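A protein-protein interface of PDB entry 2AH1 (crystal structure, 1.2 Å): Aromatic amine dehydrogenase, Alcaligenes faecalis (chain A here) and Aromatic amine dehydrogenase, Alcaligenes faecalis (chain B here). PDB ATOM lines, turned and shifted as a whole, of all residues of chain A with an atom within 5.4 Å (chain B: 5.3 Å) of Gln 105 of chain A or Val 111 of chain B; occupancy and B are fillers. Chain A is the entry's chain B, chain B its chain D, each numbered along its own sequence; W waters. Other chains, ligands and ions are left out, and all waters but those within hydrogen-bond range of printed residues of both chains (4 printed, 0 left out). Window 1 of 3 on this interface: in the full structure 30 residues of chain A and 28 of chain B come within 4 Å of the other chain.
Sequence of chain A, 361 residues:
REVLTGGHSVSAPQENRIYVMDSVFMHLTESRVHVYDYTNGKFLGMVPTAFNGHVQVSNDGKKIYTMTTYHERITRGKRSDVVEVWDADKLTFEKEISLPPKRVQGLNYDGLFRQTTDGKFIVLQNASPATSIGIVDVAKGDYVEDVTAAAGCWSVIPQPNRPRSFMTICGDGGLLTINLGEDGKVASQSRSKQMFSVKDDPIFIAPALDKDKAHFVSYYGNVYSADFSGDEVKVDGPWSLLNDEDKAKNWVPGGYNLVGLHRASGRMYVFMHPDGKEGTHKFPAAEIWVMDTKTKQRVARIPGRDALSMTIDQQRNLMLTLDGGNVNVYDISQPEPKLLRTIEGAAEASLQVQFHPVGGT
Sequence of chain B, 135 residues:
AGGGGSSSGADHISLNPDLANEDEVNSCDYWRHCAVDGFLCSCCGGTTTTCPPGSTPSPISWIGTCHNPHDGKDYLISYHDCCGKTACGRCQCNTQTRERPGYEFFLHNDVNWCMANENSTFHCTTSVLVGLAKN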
ATOM      1  N   PHE A  51       2.911 -11.960 -30.160  1.00  0.00           N
ATOM      2  CA  PHE A  51       1.728 -11.111 -30.153  1.00  0.00           C
ATOM      3  C   PHE A  51       1.804 -10.043 -29.076  1.00  0.00           C
ATOM      4  O   PHE A  51       1.844 -10.360 -27.897  1.00  0.00           O
ATOM      5  CB  PHE A  51       0.445 -11.935 -29.934  1.00  0.00           C
ATOM      6  CG  PHE A  51      -0.803 -11.119 -29.906  1.00  0.00           C
ATOM      7  CD1 PHE A  51      -1.347 -10.661 -31.084  1.00  0.00           C
ATOM      8  CD2 PHE A  51      -1.437 -10.810 -28.711  1.00  0.00           C
ATOM      9  CE1 PHE A  51      -2.481  -9.920 -31.059  1.00  0.00           C
ATOM     10  CE2 PHE A  51      -2.586 -10.059 -28.711  1.00  0.00           C
ATOM     11  CZ  PHE A  51      -3.104  -9.615 -29.881  1.00  0.00           C
ATOM     12  N   ASN A  52       1.840  -8.777 -29.484  1.00  0.00           N
ATOM     13  CA  ASN A  52       1.763  -7.662 -28.530  1.00  0.00           C
ATOM     14  C   ASN A  52       2.727  -7.781 -27.380  1.00  0.00           C
ATOM     15  O   ASN A  52       2.323  -7.775 -26.214  1.00  0.00           O
ATOM     16  CB  ASN A  52       0.333  -7.533 -27.997  1.00  0.00           C
ATOM     17  CG  ASN A  52       0.131  -6.369 -27.048  1.00  0.00           C
ATOM     18  OD1 ASN A  52       0.638  -5.248 -27.239  1.00  0.00           O
ATOM     19  ND2 ASN A  52      -0.628  -6.621 -26.027  1.00  0.00           N
ATOM     20  N   HIS A  54       5.573  -6.915 -24.596  1.00  0.00           N
ATOM     21  CA  HIS A  54       6.029  -5.870 -23.712  1.00  0.00           C
ATOM     22  C   HIS A  54       7.487  -6.163 -23.342  1.00  0.00           C
ATOM     23  O   HIS A  54       7.941  -7.308 -23.433  1.00  0.00           O
ATOM     24  CB  HIS A  54       5.140  -5.786 -22.460  1.00  0.00           C
ATOM     25  CG  HIS A  54       3.781  -5.217 -22.729  1.00  0.00           C
ATOM     26  ND1 HIS A  54       3.275  -4.115 -22.071  1.00  0.00           N
ATOM     27  CD2 HIS A  54       2.829  -5.602 -23.602  1.00  0.00           C
ATOM     28  CE1 HIS A  54       2.067  -3.852 -22.533  1.00  0.00           C
ATOM     29  NE2 HIS A  54       1.766  -4.745 -23.457  1.00  0.00           N
ATOM     30  N   THR A  69       2.340 -13.429 -25.568  1.00  0.00           N
ATOM     31  CA  THR A  69       1.345 -14.507 -25.683  1.00  0.00           C
ATOM     32  C   THR A  69       1.613 -15.311 -26.927  1.00  0.00           C
ATOM     33  O   THR A  69       1.796 -14.727 -28.017  1.00  0.00           O
ATOM     34  CB  THR A  69      -0.077 -13.913 -25.793  1.00  0.00           C
ATOM     35  OG1 THR A  69      -0.418 -13.275 -24.563  1.00  0.00           O
ATOM     36  CG2 THR A  69      -1.138 -14.992 -26.091  1.00  0.00           C
ATOM     37  N   ARG A  79      -3.298 -21.415 -25.363  1.00  0.00           N
ATOM     38  CA  ARG A  79      -2.587 -20.171 -25.021  1.00  0.00           C
ATOM     39  C   ARG A  79      -1.459 -20.376 -24.021  1.00  0.00           C
ATOM     40  O   ARG A  79      -1.635 -21.086 -23.043  1.00  0.00           O
ATOM     41  CB  ARG A  79      -3.592 -19.175 -24.425  1.00  0.00           C
ATOM     42  CG  ARG A  79      -3.031 -17.815 -24.040  1.00  0.00           C
ATOM     43  CD  ARG A  79      -4.127 -16.803 -23.877  1.00  0.00           C
ATOM     44  NE  ARG A  79      -3.685 -15.603 -23.187  1.00  0.00           N
ATOM     45  CZ  ARG A  79      -4.467 -14.553 -22.952  1.00  0.00           C
ATOM     46  NH1 ARG A  79      -5.710 -14.555 -23.384  1.00  0.00           N
ATOM     47  NH2 ARG A  79      -4.000 -13.511 -22.297  1.00  0.00           N
ATOM     48  N   ASP A  81       0.851 -17.585 -22.013  1.00  0.00           N
ATOM     49  CA  ASP A  81       1.391 -16.286 -21.644  1.00  0.00           C
ATOM     50  C   ASP A  81       2.710 -16.505 -20.902  1.00  0.00           C
ATOM     51  O   ASP A  81       2.791 -17.368 -20.040  1.00  0.00           O
ATOM     52  CB  ASP A  81       0.422 -15.523 -20.750  1.00  0.00           C
ATOM     53  CG  ASP A  81      -0.745 -14.990 -21.476  1.00  0.00           C
ATOM     54  OD1 ASP A  81      -0.858 -15.164 -22.714  1.00  0.00           O
ATOM     55  OD2 ASP A  81      -1.622 -14.387 -20.826  1.00  0.00           O
ATOM     56  N   ARG A 103      -2.210 -12.257 -18.840  1.00  0.00           N
ATOM     57  CA  ARG A 103      -1.338 -11.084 -18.864  1.00  0.00           C
ATOM     58  C   ARG A 103      -1.979  -9.987 -19.700  1.00  0.00           C
ATOM     59  O   ARG A 103      -2.669 -10.255 -20.682  1.00  0.00           O
ATOM     60  CB  ARG A 103       0.069 -11.416 -19.346  1.00  0.00           C
ATOM     61  CG  ARG A 103       0.233 -11.735 -20.821  1.00  0.00           C
ATOM     62  CD  ARG A 103       0.445 -10.519 -21.690  1.00  0.00           C
ATOM     63  NE  ARG A 103       0.605 -10.877 -23.084  1.00  0.00           N
ATOM     64  CZ  ARG A 103       0.839 -10.012 -24.055  1.00  0.00           C
ATOM     65  NH1 ARG A 103       0.910  -8.721 -23.799  1.00  0.00           N
ATOM     66  NH2 ARG A 103       1.011 -10.449 -25.306  1.00  0.00           N
ATOM     67  N   VAL A 104      -1.759  -8.732 -19.319  1.00  0.00           N
ATOM     68  CA  VAL A 104      -2.424  -7.648 -20.051  1.00  0.00           C
ATOM     69  C   VAL A 104      -2.008  -7.613 -21.514  1.00  0.00           C
ATOM     70  O   VAL A 104      -0.822  -7.620 -21.826  1.00  0.00           O
ATOM     71  CB  VAL A 104      -2.139  -6.265 -19.409  1.00  0.00           C
ATOM     72  CG1 VAL A 104      -0.654  -5.922 -19.366  1.00  0.00           C
ATOM     73  CG2 VAL A 104      -2.906  -5.179 -20.133  1.00  0.00           C
ATOM     74  N   GLN A 105      -2.982  -7.575 -22.406  1.00  0.00           N
ATOM     75  CA  GLN A 105      -2.786  -7.342 -23.817  1.00  0.00           C
ATOM     76  C   GLN A 105      -3.288  -5.912 -24.075  1.00  0.00           C
ATOM     77  O   GLN A 105      -4.475  -5.576 -23.946  1.00  0.00           O
ATOM     78  CB  GLN A 105      -3.543  -8.374 -24.626  1.00  0.00           C
ATOM     79  CG  GLN A 105      -3.003  -9.781 -24.384  1.00  0.00           C
ATOM     80  CD  GLN A 105      -3.732 -10.866 -25.132  1.00  0.00           C
ATOM     81  OE1 GLN A 105      -3.192 -12.011 -25.295  1.00  0.00           O
ATOM     82  NE2 GLN A 105      -4.913 -10.561 -25.582  1.00  0.00           N
ATOM     83  N   GLY A 106      -2.344  -5.053 -24.433  1.00  0.00           N
ATOM     84  CA  GLY A 106      -2.657  -3.649 -24.630  1.00  0.00           C
ATOM     85  C   GLY A 106      -1.414  -2.884 -25.003  1.00  0.00           C
ATOM     86  O   GLY A 106      -0.295  -3.415 -25.104  1.00  0.00           O
ATOM     87  N   LEU A 107      -1.617  -1.607 -25.204  1.00  0.00           N
ATOM     88  CA  LEU A 107      -0.537  -0.731 -25.612  1.00  0.00           C
ATOM     89  C   LEU A 107       0.522  -0.600 -24.529  1.00  0.00           C
ATOM     90  O   LEU A 107       0.271  -0.829 -23.349  1.00  0.00           O
ATOM     91  CB  LEU A 107      -1.082   0.651 -25.980  1.00  0.00           C
ATOM     92  CG  LEU A 107      -2.174   0.668 -27.045  1.00  0.00           C
ATOM     93  CD1 LEU A 107      -2.555   2.093 -27.350  1.00  0.00           C
ATOM     94  CD2 LEU A 107      -1.835  -0.082 -28.316  1.00  0.00           C
ATOM     95  N   TRP A 154      -5.224  -0.270 -11.721  1.00  0.00           N
ATOM     96  CA  TRP A 154      -4.506  -0.396 -12.989  1.00  0.00           C
ATOM     97  C   TRP A 154      -3.123   0.198 -12.902  1.00  0.00           C
ATOM     98  O   TRP A 154      -2.921   1.338 -12.461  1.00  0.00           O
ATOM     99  CB  TRP A 154      -5.296   0.312 -14.077  1.00  0.00           C
ATOM    100  CG  TRP A 154      -4.898  -0.075 -15.454  1.00  0.00           C
ATOM    101  CD1 TRP A 154      -4.310   0.721 -16.390  1.00  0.00           C
ATOM    102  CD2 TRP A 154      -5.066  -1.350 -16.060  1.00  0.00           C
ATOM    103  NE1 TRP A 154      -4.097   0.008 -17.546  1.00  0.00           N
ATOM    104  CE2 TRP A 154      -4.553  -1.268 -17.370  1.00  0.00           C
ATOM    105  CE3 TRP A 154      -5.591  -2.565 -15.628  1.00  0.00           C
ATOM    106  CZ2 TRP A 154      -4.559  -2.357 -18.245  1.00  0.00           C
ATOM    107  CZ3 TRP A 154      -5.601  -3.628 -16.488  1.00  0.00           C
ATOM    108  CH2 TRP A 154      -5.080  -3.523 -17.784  1.00  0.00           C
ATOM    109  N   TRQ B  62     -15.188  -2.557 -24.449  1.00  0.00           N
ATOM    110  CA  TRQ B  62     -15.235  -1.215 -23.884  1.00  0.00           C
ATOM    111  C   TRQ B  62     -16.500  -0.535 -24.424  1.00  0.00           C
ATOM    112  O   TRQ B  62     -17.028  -0.903 -25.471  1.00  0.00           O
ATOM    113  CB  TRQ B  62     -13.920  -0.423 -24.146  1.00  0.00           C
ATOM    114  CG  TRQ B  62     -13.528  -0.175 -25.601  1.00  0.00           C
ATOM    115  CD1 TRQ B  62     -13.851   0.926 -26.291  1.00  0.00           C
ATOM    116  NE1 TRQ B  62     -13.380   0.857 -27.571  1.00  0.00           N
ATOM    117  CE2 TRQ B  62     -12.713  -0.323 -27.751  1.00  0.00           C
ATOM    118  CZ2 TRQ B  62     -12.077  -0.815 -28.901  1.00  0.00           C
ATOM    119  CH2 TRQ B  62     -11.485  -2.038 -28.815  1.00  0.00           C
ATOM    120  CZ3 TRQ B  62     -11.508  -2.778 -27.614  1.00  0.00           C
ATOM    121  CE3 TRQ B  62     -12.147  -2.290 -26.473  1.00  0.00           C
ATOM    122  CD2 TRQ B  62     -12.771  -1.024 -26.540  1.00  0.00           C
ATOM    123  O6  TRQ B  62     -10.935  -2.519 -29.881  1.00  0.00           O
ATOM    124  O7  TRQ B  62     -12.084  -0.064 -29.959  1.00  0.00           O
ATOM    125  N   ASP B  81     -15.012  -6.747 -29.929  1.00  0.00           N
ATOM    126  CA  ASP B  81     -14.068  -7.100 -30.970  1.00  0.00           C
ATOM    127  C   ASP B  81     -14.502  -8.368 -31.646  1.00  0.00           C
ATOM    128  O   ASP B  81     -15.344  -9.115 -31.143  1.00  0.00           O
ATOM    129  CB  ASP B  81     -12.659  -7.279 -30.406  1.00  0.00           C
ATOM    130  CG  ASP B  81     -12.033  -6.000 -29.972  1.00  0.00           C
ATOM    131  OD1 ASP B  81     -12.414  -4.905 -30.490  1.00  0.00           O
ATOM    132  OD2 ASP B  81     -11.120  -6.000 -29.118  1.00  0.00           O
ATOM    133  N   PHE B 105     -12.074   0.555 -16.271  1.00  0.00           N
ATOM    134  CA  PHE B 105     -11.529  -0.402 -17.235  1.00  0.00           C
ATOM    135  C   PHE B 105     -12.407  -0.556 -18.457  1.00  0.00           C
ATOM    136  O   PHE B 105     -11.912  -0.635 -19.569  1.00  0.00           O
ATOM    137  CB  PHE B 105     -11.302  -1.752 -16.567  1.00  0.00           C
ATOM    138  CG  PHE B 105     -10.361  -2.659 -17.332  1.00  0.00           C
ATOM    139  CD1 PHE B 105      -9.130  -2.212 -17.810  1.00  0.00           C
ATOM    140  CD2 PHE B 105     -10.712  -3.961 -17.556  1.00  0.00           C
ATOM    141  CE1 PHE B 105      -8.285  -3.059 -18.509  1.00  0.00           C
ATOM    142  CE2 PHE B 105      -9.872  -4.810 -18.248  1.00  0.00           C
ATOM    143  CZ  PHE B 105      -8.658  -4.355 -18.721  1.00  0.00           C
ATOM    144  N   HIS B 108     -12.132   1.917 -21.383  1.00  0.00           N
ATOM    145  CA  HIS B 108     -10.754   2.061 -21.828  1.00  0.00           C
ATOM    146  C   HIS B 108     -10.504   1.308 -23.128  1.00  0.00           C
ATOM    147  O   HIS B 108     -10.911   0.157 -23.264  1.00  0.00           O
ATOM    148  CB  HIS B 108      -9.834   1.515 -20.724  1.00  0.00           C
ATOM    149  CG  HIS B 108      -8.383   1.720 -21.006  1.00  0.00           C
ATOM    150  ND1 HIS B 108      -7.407   0.760 -20.840  1.00  0.00           N
ATOM    151  CD2 HIS B 108      -7.755   2.824 -21.448  1.00  0.00           C
ATOM    152  CE1 HIS B 108      -6.232   1.267 -21.182  1.00  0.00           C
ATOM    153  NE2 HIS B 108      -6.426   2.522 -21.556  1.00  0.00           N
ATOM    154  N   ASN B 109      -9.817   1.943 -24.080  1.00  0.00           N
ATOM    155  CA  ASN B 109      -9.625   1.310 -25.400  1.00  0.00           C
ATOM    156  C   ASN B 109      -8.169   1.050 -25.818  1.00  0.00           C
ATOM    157  O   ASN B 109      -7.921   0.758 -26.969  1.00  0.00           O
ATOM    158  CB  ASN B 109     -10.400   2.027 -26.522  1.00  0.00           C
ATOM    159  CG  ASN B 109      -9.818   3.347 -26.927  1.00  0.00           C
ATOM    160  OD1 ASN B 109      -8.715   3.707 -26.528  1.00  0.00           O
ATOM    161  ND2 ASN B 109     -10.575   4.099 -27.746  1.00  0.00           N
ATOM    162  N   ASP B 110      -7.244   1.137 -24.870  1.00  0.00           N
ATOM    163  CA  ASP B 110      -5.861   0.759 -25.152  1.00  0.00           C
ATOM    164  C   ASP B 110      -5.525  -0.667 -24.708  1.00  0.00           C
ATOM    165  O   ASP B 110      -4.347  -1.020 -24.525  1.00  0.00           O
ATOM    166  CB  ASP B 110      -4.865   1.688 -24.461  1.00  0.00           C
ATOM    167  CG  ASP B 110      -4.981   3.119 -24.880  1.00  0.00           C
ATOM    168  OD1 ASP B 110      -5.455   3.401 -25.991  1.00  0.00           O
ATOM    169  OD2 ASP B 110      -4.584   4.014 -24.118  1.00  0.00           O
ATOM    170  N   VAL B 111      -6.550  -1.479 -24.542  1.00  0.00           N
ATOM    171  CA  VAL B 111      -6.422  -2.899 -24.264  1.00  0.00           C
ATOM    172  C   VAL B 111      -7.225  -3.684 -25.296  1.00  0.00           C
ATOM    173  O   VAL B 111      -8.135  -3.169 -25.939  1.00  0.00           O
ATOM    174  CB  VAL B 111      -6.884  -3.283 -22.830  1.00  0.00           C
ATOM    175  CG1 VAL B 111      -5.960  -2.673 -21.817  1.00  0.00           C
ATOM    176  CG2 VAL B 111      -8.338  -2.870 -22.548  1.00  0.00           C
ATOM    177  N   ASN B 112      -6.848  -4.945 -25.448  1.00  0.00           N
ATOM    178  CA  ASN B 112      -7.447  -5.841 -26.423  1.00  0.00           C
ATOM    179  C   ASN B 112      -8.712  -6.450 -25.864  1.00  0.00           C
ATOM    180  O   ASN B 112      -8.630  -7.286 -24.960  1.00  0.00           O
ATOM    181  CB  ASN B 112      -6.425  -6.953 -26.681  1.00  0.00           C
ATOM    182  CG  ASN B 112      -6.895  -7.982 -27.674  1.00  0.00           C
ATOM    183  OD1 ASN B 112      -7.820  -7.759 -28.465  1.00  0.00           O
ATOM    184  ND2 ASN B 112      -6.244  -9.144 -27.653  1.00  0.00           N
ATOM    185  N   TRP B 113      -9.884  -6.058 -26.377  1.00  0.00           N
ATOM    186  CA  TRP B 113     -11.134  -6.624 -25.861  1.00  0.00           C
ATOM    187  C   TRP B 113     -11.344  -8.085 -26.275  1.00  0.00           C
ATOM    188  O   TRP B 113     -12.313  -8.696 -25.829  1.00  0.00           O
ATOM    189  CB  TRP B 113     -12.388  -5.681 -26.004  1.00  0.00           C
ATOM    190  CG  TRP B 113     -12.213  -4.578 -25.037  1.00  0.00           C
ATOM    191  CD1 TRP B 113     -12.012  -3.280 -25.288  1.00  0.00           C
ATOM    192  CD2 TRP B 113     -12.201  -4.710 -23.607  1.00  0.00           C
ATOM    193  NE1 TRP B 113     -11.833  -2.588 -24.112  1.00  0.00           N
ATOM    194  CE2 TRP B 113     -11.968  -3.450 -23.062  1.00  0.00           C
ATOM    195  CE3 TRP B 113     -12.376  -5.780 -22.742  1.00  0.00           C
ATOM    196  CZ2 TRP B 113     -11.905  -3.227 -21.692  1.00  0.00           C
ATOM    197  CZ3 TRP B 113     -12.313  -5.568 -21.385  1.00  0.00           C
ATOM    198  CH2 TRP B 113     -12.079  -4.297 -20.873  1.00  0.00           C
ATOM    199  N   CYS B 114     -10.413  -8.645 -27.080  1.00  0.00           N
ATOM    200  CA  CYS B 114     -10.357 -10.089 -27.306  1.00  0.00           C
ATOM    201  C   CYS B 114      -9.647 -10.862 -26.197  1.00  0.00           C
ATOM    202  O   CYS B 114      -9.477 -12.068 -26.305  1.00  0.00           O
ATOM    203  CB  CYS B 114      -9.600 -10.389 -28.600  1.00  0.00           C
ATOM    204  SG  CYS B 114     -10.438  -9.856 -30.112  1.00  0.00           S
ATOM    205  N   MET B 115      -9.209 -10.173 -25.144  1.00  0.00           N
ATOM    206  CA  MET B 115      -8.310 -10.777 -24.148  1.00  0.00           C
ATOM    207  C   MET B 115      -8.804 -12.028 -23.456  1.00  0.00           C
ATOM    208  O   MET B 115      -7.981 -12.802 -22.941  1.00  0.00           O
ATOM    209  CB  MET B 115      -7.962  -9.755 -23.049  1.00  0.00           C
ATOM    210  CG  MET B 115      -9.161  -9.334 -22.186  1.00  0.00           C
ATOM    211  SD  MET B 115      -8.773  -8.067 -20.955  1.00  0.00           S
ATOM    212  CE  MET B 115      -8.923  -6.557 -21.909  1.00  0.00           C
ATOM    213  N   SER B 120      -7.172 -14.965 -28.514  1.00  0.00           N
ATOM    214  CA  SER B 120      -7.133 -13.536 -28.255  1.00  0.00           C
ATOM    215  C   SER B 120      -6.573 -12.688 -29.405  1.00  0.00           C
ATOM    216  O   SER B 120      -6.469 -11.495 -29.250  1.00  0.00           O
ATOM    217  CB  SER B 120      -6.349 -13.276 -26.965  1.00  0.00           C
ATOM    218  OG  SER B 120      -5.057 -13.842 -26.999  1.00  0.00           O
HETATM  219  O   HOH W   1      -6.531 -16.438 -25.958  1.00  0.00           O
HETATM  220  O   HOH W   2      -8.682 -15.887 -22.816  1.00  0.00           O
HETATM  221  O   HOH W   3      -2.556  -0.500 -22.430  1.00  0.00           O
HETATM  222  O   HOH W   4      -5.528  -7.795 -21.425  1.00  0.00           O
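The side-chain amide nitrogen (ND2) of Asn 112 of chain B sits close to the side-chain amide nitrogen (NE2) of Gln 105 of chain A.
The backbone carbonyl oxygen (O) of Met 115 of chain B sits at hydrogen-bond distance from the guanidinium group (NH1) of Arg 79 of chain A.
The backbone carbonyl oxygen of Asp 110 of chain B lies within hydrogen-bond range of the backbone NH of Leu 107 of chain A.
OG of Ser 120 of chain B is in hydrogen-bond range of OE1 of Gln 105 of chain A (3.1 Å).
The side-chain carboxylate (OD1) of Asp 81 of chain A lies within salt-bridge range of the guanidinium group (NE) of Arg 79 of chain A (2.9 Å).
ND2 of Asn 52 of chain A sits close to N of Gly 106 of chain A (2.8 Å).
The guanidinium group (NH2) of Arg 79 of chain A lies within hydrogen-bond range of the side-chain amide oxygen (OE1) of Gln 105 of chain A, at 3.4 Å.
The side-chain amide oxygen (OD1) of Asn 109 of chain B sits close to the side-chain carboxylate (OD1) of Asp 110 of chain B (3.3 Å).
OG1 of Thr 69 of chain A is in hydrogen-bond range of OE1 of Gln 105 of chain A, at 3.1 Å.
N of Cys 114 of chain B lies close to OD1 of Asn 112 of chain B (3.1 Å).
Phe 51 of chain A touches Asn 112 of chain B (CZ to ND2, 3.9 Å).
Ser 120 of chain B touches Phe 51 of chain A (O to CZ, 3.9 Å).
Arg 79 of chain A touches Ser 120 of chain B (NH1 to OG, 3.7 Å).
Val 111 of chain B touches Gln 105 of chain A (CA to O, 3.3 Å).
Gln 105 of chain A touches Met 115 of chain B.
Gly 106 of chain A touches Asp 110 of chain B.
CA of Gly 106 of chain A touches CA of Val 111 of chain B, at 3.9 Å.
CH2 of Trp 154 of chain A touches CE1 of Phe 105 of chain B, 3.3 Å away.
Trp 154 of chain A touches Val 111 of chain B.
Thr 69 of chain A touches none of the printed residues of chain B.
Of the printed residues of chain B, Arg 79 of chain A touches Met 115 (2.9 Å) and Ser 120 (3.7 Å).
Of chain B, only Val 111 (3.3 Å), Asn 112 (2.8 Å), Met 115 (3.7 Å) and Ser 120 (3.1 Å) come within 4 Å of Gln 105 of chain A.
Printed residues of chain B within 4 Å of Leu 107 of chain A: Asp 110.
Of the printed residues of chain A, Asp 110 of chain B touches Gly 106 and Leu 107.
Printed residues of chain A within 4 Å of Met 115 of chain B: Arg 79 (2.9 Å) and Gln 105 (3.7 Å).
Of the printed residues of chain A, Ser 120 of chain B touches Phe 51 (3.9 Å), Arg 79 (3.7 Å) and Gln 105 (3.1 Å).
The nearest residue of chain A that does not touch Val 111 of chain B is Val 104 of chain A (4.3 Å).
Hydrophobic or aromatic side chains of chain A within 4 Å of the printed part of chain B: Phe 51, Leu 107 and Trp 154.
Among the printed residues, 13 pairs touch across the chains.
Among the printed residues, no Asp or Glu carboxylate lies within 4 Å of a Lys or Arg side-chain nitrogen of the other chain.
Water W4 lies within hydrogen-bond range of N of Gln 105 of chain A (2.7 Å) and SD of Met 115 of chain B (3.3 Å).
Water W3 lies within hydrogen-bond range of the backbone carbonyl oxygen (O) of Asp 110 of chain B (2.8 Å) and the backbone carbonyl oxygen (O) of Leu 107 of chain A (3.0 Å).
Water W1 bridges the backbone NH (N) of Ser 120 of chain B (3.0 Å) and the guanidinium group (NH1) of Arg 79 of chain A (3.3 Å).
Water W2 lies within hydrogen-bond range of O of Met 115 of chain B (3.2 Å) and NH1 of Arg 79 of chain A (3.3 Å).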
